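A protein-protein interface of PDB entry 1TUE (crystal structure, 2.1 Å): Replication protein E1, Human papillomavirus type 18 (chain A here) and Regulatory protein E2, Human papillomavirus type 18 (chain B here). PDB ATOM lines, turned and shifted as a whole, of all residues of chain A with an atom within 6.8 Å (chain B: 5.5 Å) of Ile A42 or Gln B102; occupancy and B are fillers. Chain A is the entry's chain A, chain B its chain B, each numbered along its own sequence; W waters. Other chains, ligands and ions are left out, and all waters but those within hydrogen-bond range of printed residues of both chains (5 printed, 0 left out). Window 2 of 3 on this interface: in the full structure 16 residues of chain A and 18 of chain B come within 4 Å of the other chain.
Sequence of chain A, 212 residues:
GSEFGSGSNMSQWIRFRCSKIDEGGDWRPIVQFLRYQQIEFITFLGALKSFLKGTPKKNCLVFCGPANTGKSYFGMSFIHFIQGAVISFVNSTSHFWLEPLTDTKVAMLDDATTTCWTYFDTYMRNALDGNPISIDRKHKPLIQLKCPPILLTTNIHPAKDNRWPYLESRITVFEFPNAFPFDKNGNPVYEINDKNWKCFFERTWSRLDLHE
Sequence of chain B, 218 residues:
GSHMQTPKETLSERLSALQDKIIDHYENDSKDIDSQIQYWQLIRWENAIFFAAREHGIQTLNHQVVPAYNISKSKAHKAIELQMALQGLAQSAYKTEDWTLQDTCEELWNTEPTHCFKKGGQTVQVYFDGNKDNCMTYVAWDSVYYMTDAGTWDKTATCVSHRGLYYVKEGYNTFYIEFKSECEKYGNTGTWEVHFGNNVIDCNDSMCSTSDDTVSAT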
ATOM      1  N   ILE A  39      27.511   8.729  26.298  1.00  0.00           N
ATOM      2  CA  ILE A  39      26.053   8.705  26.235  1.00  0.00           C
ATOM      3  C   ILE A  39      25.660   7.658  25.190  1.00  0.00           C
ATOM      4  O   ILE A  39      26.279   7.577  24.121  1.00  0.00           O
ATOM      5  CB  ILE A  39      25.507  10.128  25.916  1.00  0.00           C
ATOM      6  CG1 ILE A  39      25.833  11.089  27.074  1.00  0.00           C
ATOM      7  CG2 ILE A  39      24.011  10.096  25.629  1.00  0.00           C
ATOM      8  CD1 ILE A  39      25.629  12.589  26.776  1.00  0.00           C
ATOM      9  N   GLU A  40      24.686   6.823  25.527  1.00  0.00           N
ATOM     10  CA  GLU A  40      24.170   5.837  24.589  1.00  0.00           C
ATOM     11  C   GLU A  40      23.240   6.521  23.594  1.00  0.00           C
ATOM     12  O   GLU A  40      22.278   7.187  23.993  1.00  0.00           O
ATOM     13  CB  GLU A  40      23.391   4.724  25.315  1.00  0.00           C
ATOM     14  CG  GLU A  40      24.232   3.648  25.990  1.00  0.00           C
ATOM     15  CD  GLU A  40      25.139   2.894  25.036  1.00  0.00           C
ATOM     16  OE1 GLU A  40      24.779   2.737  23.836  1.00  0.00           O
ATOM     17  OE2 GLU A  40      26.226   2.459  25.491  1.00  0.00           O
ATOM     18  N   PHE A  41      23.534   6.342  22.308  1.00  0.00           N
ATOM     19  CA  PHE A  41      22.712   6.888  21.223  1.00  0.00           C
ATOM     20  C   PHE A  41      21.223   6.589  21.387  1.00  0.00           C
ATOM     21  O   PHE A  41      20.416   7.509  21.376  1.00  0.00           O
ATOM     22  CB  PHE A  41      23.200   6.417  19.830  1.00  0.00           C
ATOM     23  CG  PHE A  41      22.268   6.799  18.697  1.00  0.00           C
ATOM     24  CD1 PHE A  41      22.158   8.125  18.284  1.00  0.00           C
ATOM     25  CD2 PHE A  41      21.477   5.842  18.079  1.00  0.00           C
ATOM     26  CE1 PHE A  41      21.270   8.492  17.266  1.00  0.00           C
ATOM     27  CE2 PHE A  41      20.577   6.193  17.048  1.00  0.00           C
ATOM     28  CZ  PHE A  41      20.487   7.529  16.645  1.00  0.00           C
ATOM     29  N   ILE A  42      20.869   5.312  21.547  1.00  0.00           N
ATOM     30  CA  ILE A  42      19.455   4.928  21.585  1.00  0.00           C
ATOM     31  C   ILE A  42      18.755   5.573  22.780  1.00  0.00           C
ATOM     32  O   ILE A  42      17.633   6.050  22.653  1.00  0.00           O
ATOM     33  CB  ILE A  42      19.268   3.372  21.562  1.00  0.00           C
ATOM     34  CG1 ILE A  42      19.854   2.762  20.276  1.00  0.00           C
ATOM     35  CG2 ILE A  42      17.787   2.995  21.749  1.00  0.00           C
ATOM     36  CD1 ILE A  42      19.137   3.149  18.975  1.00  0.00           C
ATOM     37  N   THR A  43      19.433   5.601  23.933  1.00  0.00           N
ATOM     38  CA  THR A  43      18.908   6.281  25.121  1.00  0.00           C
ATOM     39  C   THR A  43      18.646   7.762  24.849  1.00  0.00           C
ATOM     40  O   THR A  43      17.588   8.280  25.166  1.00  0.00           O
ATOM     41  CB  THR A  43      19.882   6.137  26.310  1.00  0.00           C
ATOM     42  OG1 THR A  43      20.101   4.744  26.597  1.00  0.00           O
ATOM     43  CG2 THR A  43      19.249   6.709  27.592  1.00  0.00           C
ATOM     44  N   PHE A  44      19.628   8.447  24.276  1.00  0.00           N
ATOM     45  CA  PHE A  44      19.478   9.874  23.939  1.00  0.00           C
ATOM     46  C   PHE A  44      18.309  10.129  22.982  1.00  0.00           C
ATOM     47  O   PHE A  44      17.516  11.047  23.181  1.00  0.00           O
ATOM     48  CB  PHE A  44      20.786  10.445  23.367  1.00  0.00           C
ATOM     49  CG  PHE A  44      20.685  11.902  22.979  1.00  0.00           C
ATOM     50  CD1 PHE A  44      20.853  12.910  23.935  1.00  0.00           C
ATOM     51  CD2 PHE A  44      20.397  12.265  21.666  1.00  0.00           C
ATOM     52  CE1 PHE A  44      20.742  14.256  23.591  1.00  0.00           C
ATOM     53  CE2 PHE A  44      20.277  13.626  21.302  1.00  0.00           C
ATOM     54  CZ  PHE A  44      20.444  14.615  22.267  1.00  0.00           C
ATOM     55  N   LEU A  45      18.213   9.310  21.935  1.00  0.00           N
ATOM     56  CA  LEU A  45      17.174   9.481  20.922  1.00  0.00           C
ATOM     57  C   LEU A  45      15.789   9.269  21.538  1.00  0.00           C
ATOM     58  O   LEU A  45      14.854  10.025  21.259  1.00  0.00           O
ATOM     59  CB  LEU A  45      17.432   8.524  19.735  1.00  0.00           C
ATOM     60  CG  LEU A  45      16.616   8.738  18.456  1.00  0.00           C
ATOM     61  CD1 LEU A  45      17.033  10.045  17.783  1.00  0.00           C
ATOM     62  CD2 LEU A  45      16.801   7.571  17.502  1.00  0.00           C
ATOM     63  N   GLY A  46      15.666   8.265  22.409  1.00  0.00           N
ATOM     64  CA  GLY A  46      14.424   8.067  23.153  1.00  0.00           C
ATOM     65  C   GLY A  46      14.090   9.293  23.983  1.00  0.00           C
ATOM     66  O   GLY A  46      12.947   9.741  24.020  1.00  0.00           O
ATOM     67  N   ALA A  47      15.096   9.852  24.659  1.00  0.00           N
ATOM     68  CA  ALA A  47      14.860  11.049  25.481  1.00  0.00           C
ATOM     69  C   ALA A  47      14.440  12.241  24.627  1.00  0.00           C
ATOM     70  O   ALA A  47      13.566  13.013  25.017  1.00  0.00           O
ATOM     71  CB  ALA A  47      16.084  11.388  26.303  1.00  0.00           C
ATOM     72  N   LYS A  49      12.949  12.202  21.683  1.00  0.00           N
ATOM     73  CA  LYS A  49      11.606  11.940  21.161  1.00  0.00           C
ATOM     74  C   LYS A  49      10.554  12.414  22.169  1.00  0.00           C
ATOM     75  O   LYS A  49       9.652  13.176  21.819  1.00  0.00           O
ATOM     76  CB  LYS A  49      11.441  10.445  20.849  1.00  0.00           C
ATOM     77  CG  LYS A  49      10.002   9.967  20.525  1.00  0.00           C
ATOM     78  CD  LYS A  49      10.007   8.463  20.163  1.00  0.00           C
ATOM     79  CE  LYS A  49       8.612   7.840  20.189  1.00  0.00           C
ATOM     80  NZ  LYS A  49       8.678   6.319  20.243  1.00  0.00           N
ATOM     81  N   ARG A 207      11.920   7.469  13.849  1.00  0.00           N
ATOM     82  CA  ARG A 207      12.276   7.059  15.214  1.00  0.00           C
ATOM     83  C   ARG A 207      12.000   8.140  16.261  1.00  0.00           C
ATOM     84  O   ARG A 207      11.879   7.836  17.440  1.00  0.00           O
ATOM     85  CB  ARG A 207      13.734   6.617  15.290  1.00  0.00           C
ATOM     86  CG  ARG A 207      13.976   5.233  14.706  1.00  0.00           C
ATOM     87  CD  ARG A 207      15.433   4.852  14.640  1.00  0.00           C
ATOM     88  NE  ARG A 207      16.185   5.565  13.599  1.00  0.00           N
ATOM     89  CZ  ARG A 207      17.483   5.367  13.344  1.00  0.00           C
ATOM     90  NH1 ARG A 207      18.186   4.490  14.063  1.00  0.00           N
ATOM     91  NH2 ARG A 207      18.086   6.045  12.372  1.00  0.00           N
ATOM     92  N   TYR B  26      23.320   2.451  13.277  1.00  0.00           N
ATOM     93  CA  TYR B  26      22.366   3.483  13.677  1.00  0.00           C
ATOM     94  C   TYR B  26      21.698   4.113  12.460  1.00  0.00           C
ATOM     95  O   TYR B  26      20.503   4.385  12.478  1.00  0.00           O
ATOM     96  CB  TYR B  26      23.060   4.573  14.512  1.00  0.00           C
ATOM     97  CG  TYR B  26      23.627   4.105  15.842  1.00  0.00           C
ATOM     98  CD1 TYR B  26      23.059   3.034  16.538  1.00  0.00           C
ATOM     99  CD2 TYR B  26      24.713   4.760  16.417  1.00  0.00           C
ATOM    100  CE1 TYR B  26      23.574   2.616  17.761  1.00  0.00           C
ATOM    101  CE2 TYR B  26      25.244   4.344  17.646  1.00  0.00           C
ATOM    102  CZ  TYR B  26      24.676   3.277  18.299  1.00  0.00           C
ATOM    103  OH  TYR B  26      25.189   2.874  19.495  1.00  0.00           O
ATOM    104  N   THR B 100      14.635  -4.578  15.965  1.00  0.00           N
ATOM    105  CA  THR B 100      15.329  -3.319  15.734  1.00  0.00           C
ATOM    106  C   THR B 100      16.318  -3.021  16.862  1.00  0.00           C
ATOM    107  O   THR B 100      16.314  -3.686  17.906  1.00  0.00           O
ATOM    108  CB  THR B 100      14.336  -2.145  15.650  1.00  0.00           C
ATOM    109  OG1 THR B 100      13.649  -2.017  16.906  1.00  0.00           O
ATOM    110  CG2 THR B 100      13.230  -2.389  14.599  1.00  0.00           C
ATOM    111  N   LEU B 101      17.147  -2.002  16.638  1.00  0.00           N
ATOM    112  CA  LEU B 101      18.026  -1.449  17.677  1.00  0.00           C
ATOM    113  C   LEU B 101      17.241  -1.097  18.931  1.00  0.00           C
ATOM    114  O   LEU B 101      17.689  -1.357  20.052  1.00  0.00           O
ATOM    115  CB  LEU B 101      18.731  -0.182  17.148  1.00  0.00           C
ATOM    116  CG  LEU B 101      19.850  -0.386  16.120  1.00  0.00           C
ATOM    117  CD1 LEU B 101      20.003   0.832  15.208  1.00  0.00           C
ATOM    118  CD2 LEU B 101      21.170  -0.709  16.824  1.00  0.00           C
ATOM    119  N   GLN B 102      16.079  -0.480  18.731  1.00  0.00           N
ATOM    120  CA  GLN B 102      15.206  -0.089  19.827  1.00  0.00           C
ATOM    121  C   GLN B 102      14.657  -1.288  20.610  1.00  0.00           C
ATOM    122  O   GLN B 102      14.617  -1.246  21.840  1.00  0.00           O
ATOM    123  CB  GLN B 102      14.065   0.793  19.313  1.00  0.00           C
ATOM    124  CG  GLN B 102      13.235   1.435  20.429  1.00  0.00           C
ATOM    125  CD  GLN B 102      14.002   2.545  21.138  1.00  0.00           C
ATOM    126  OE1 GLN B 102      14.542   3.440  20.480  1.00  0.00           O
ATOM    127  NE2 GLN B 102      14.058   2.487  22.476  1.00  0.00           N
ATOM    128  N   ASP B 103      14.247  -2.346  19.895  1.00  0.00           N
ATOM    129  CA  ASP B 103      13.732  -3.568  20.513  1.00  0.00           C
ATOM    130  C   ASP B 103      14.829  -4.258  21.325  1.00  0.00           C
ATOM    131  O   ASP B 103      14.537  -5.019  22.231  1.00  0.00           O
ATOM    132  CB  ASP B 103      13.278  -4.594  19.458  1.00  0.00           C
ATOM    133  CG  ASP B 103      12.068  -4.152  18.647  1.00  0.00           C
ATOM    134  OD1 ASP B 103      11.132  -3.554  19.225  1.00  0.00           O
ATOM    135  OD2 ASP B 103      11.964  -4.415  17.408  1.00  0.00           O
ATOM    136  N   THR B 104      16.092  -4.011  20.977  1.00  0.00           N
ATOM    137  CA  THR B 104      17.188  -4.797  21.529  1.00  0.00           C
ATOM    138  C   THR B 104      18.254  -3.963  22.222  1.00  0.00           C
ATOM    139  O   THR B 104      19.385  -4.409  22.343  1.00  0.00           O
ATOM    140  CB  THR B 104      17.841  -5.663  20.428  1.00  0.00           C
ATOM    141  OG1 THR B 104      18.248  -4.817  19.347  1.00  0.00           O
ATOM    142  CG2 THR B 104      16.801  -6.606  19.780  1.00  0.00           C
ATOM    143  N   CYS B 105      17.885  -2.764  22.668  1.00  0.00           N
ATOM    144  CA  CYS B 105      18.816  -1.869  23.356  1.00  0.00           C
ATOM    145  C   CYS B 105      18.930  -2.259  24.827  1.00  0.00           C
ATOM    146  O   CYS B 105      18.065  -2.962  25.352  1.00  0.00           O
ATOM    147  CB  CYS B 105      18.373  -0.400  23.216  1.00  0.00           C
ATOM    148  SG  CYS B 105      16.926   0.061  24.203  1.00  0.00           S
ATOM    149  N   GLU B 107      18.729  -0.327  27.502  1.00  0.00           N
ATOM    150  CA  GLU B 107      17.695   0.366  28.277  1.00  0.00           C
ATOM    151  C   GLU B 107      16.438  -0.485  28.429  1.00  0.00           C
ATOM    152  O   GLU B 107      15.908  -0.617  29.531  1.00  0.00           O
ATOM    153  CB  GLU B 107      17.370   1.714  27.619  1.00  0.00           C
ATOM    154  CG  GLU B 107      16.388   2.627  28.353  1.00  0.00           C
ATOM    155  CD  GLU B 107      16.182   3.949  27.625  1.00  0.00           C
ATOM    156  OE1 GLU B 107      16.211   3.971  26.370  1.00  0.00           O
ATOM    157  OE2 GLU B 107      15.991   4.978  28.300  1.00  0.00           O
ATOM    158  N   LEU B 108      15.964  -1.063  27.323  1.00  0.00           N
ATOM    159  CA  LEU B 108      14.777  -1.916  27.354  1.00  0.00           C
ATOM    160  C   LEU B 108      15.063  -3.246  28.065  1.00  0.00           C
ATOM    161  O   LEU B 108      14.249  -3.721  28.859  1.00  0.00           O
ATOM    162  CB  LEU B 108      14.227  -2.139  25.933  1.00  0.00           C
ATOM    163  CG  LEU B 108      12.901  -2.894  25.764  1.00  0.00           C
ATOM    164  CD1 LEU B 108      11.805  -2.325  26.672  1.00  0.00           C
ATOM    165  CD2 LEU B 108      12.448  -2.875  24.308  1.00  0.00           C
HETATM  166  O   HOH W   1      25.676   4.455  21.510  1.00  0.00           O
HETATM  167  O   HOH W   2      22.696   3.150  21.812  1.00  0.00           O
HETATM  168  O   HOH W   3      15.012   4.637  23.829  1.00  0.00           O
HETATM  169  O   HOH W   4      19.719   1.723  25.479  1.00  0.00           O
HETATM  170  O   HOH W   5      15.688   7.275  26.805  1.00  0.00           O
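Water W1 lies within hydrogen-bond range of the side-chain hydroxyl of Tyr B26 (2.6 Å), the backbone NH of Phe A41 (3.0 Å) and the side-chain carboxylate of Glu A40 (3.0 Å).
Water W5 lies within hydrogen-bond range of the backbone carbonyl oxygen (O) of Thr A43 (2.7 Å), the side-chain carboxylate (OE2) of Glu B107 (2.8 Å) and the backbone NH (N) of Ala A47 (3.4 Å).
Water W3 lies within hydrogen-bond range of NE2 of Gln B102 (2.7 Å), OE1 of Glu B107 (2.9 Å) and O of Ile A42 (3.2 Å).
Water W2 lies within hydrogen-bond range of N of Ile A42 (2.8 Å), OE1 of Glu A40 (2.9 Å), N of Phe A41 (3.3 Å) and OH of Tyr B26 (3.4 Å).
Water W4 lies within hydrogen-bond range of N of Glu B107, OG1 of Thr A43 and SG of Cys B105.
The side-chain sulfur of Cys B105 lies close to the backbone NH of Glu B107, at 3.8 Å.
The side-chain sulfur (SG) of Cys B105 is in hydrogen-bond range of the backbone NH (N) of Leu B108, 3.5 Å away.
SG of Cys B105 is in hydrogen-bond range of O of Gln B102 (3.6 Å).
The backbone NH of Gln B102 sits close to the side-chain hydroxyl of Thr B100 (3.4 Å).
The backbone carbonyl oxygen (O) of Tyr B26 lies within hydrogen-bond range of the guanidinium group (NH1) of Arg A207 (2.8 Å).
Tyr B26 touches Phe A41 (CG to CD2, 3.6 Å).
Leu B101 touches Ile A42.
Ile A42 touches Gln B102.
Ile A42 touches Cys B105.
OE2 of Glu B107 touches CG2 of Thr A43, 3.8 Å away.
Of the 11 printed residues of chain A, 4 touch a printed residue of chain B.
Along chain B the printed residues that touch a printed residue of chain A span positions 26 to 107.
Among the printed residues, no Asp or Glu carboxylate lies within 4 Å of a Lys or Arg side-chain nitrogen of the other chain.
Ile A42 touches three residues of chain B.
Gln B102 touches just one residue of chain A: Ile A42 (3.5 Å).
Of the printed residues of chain B, Thr A43 touches Glu B107.
Printed residues of chain A within 4 Å of Tyr B26: Phe A41 and Arg A207.
Printed residues of chain B within 4 Å of Phe A41: Tyr B26 (3.6 Å).
Of the printed residues of chain B, Arg A207 touches Tyr B26.
Printed residues of chain A within 4 Å of Glu B107: Thr A43.
Ile A39 touches none of the printed residues of chain B.
Thr B104 touches none of the printed residues of chain A.
The nearest printed residue of chain B that does not touch Ile A42 is Glu B107 (4.5 Å).
The nearest residue of chain A that does not touch Gln B102 is Gly A46 (5.3 Å).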
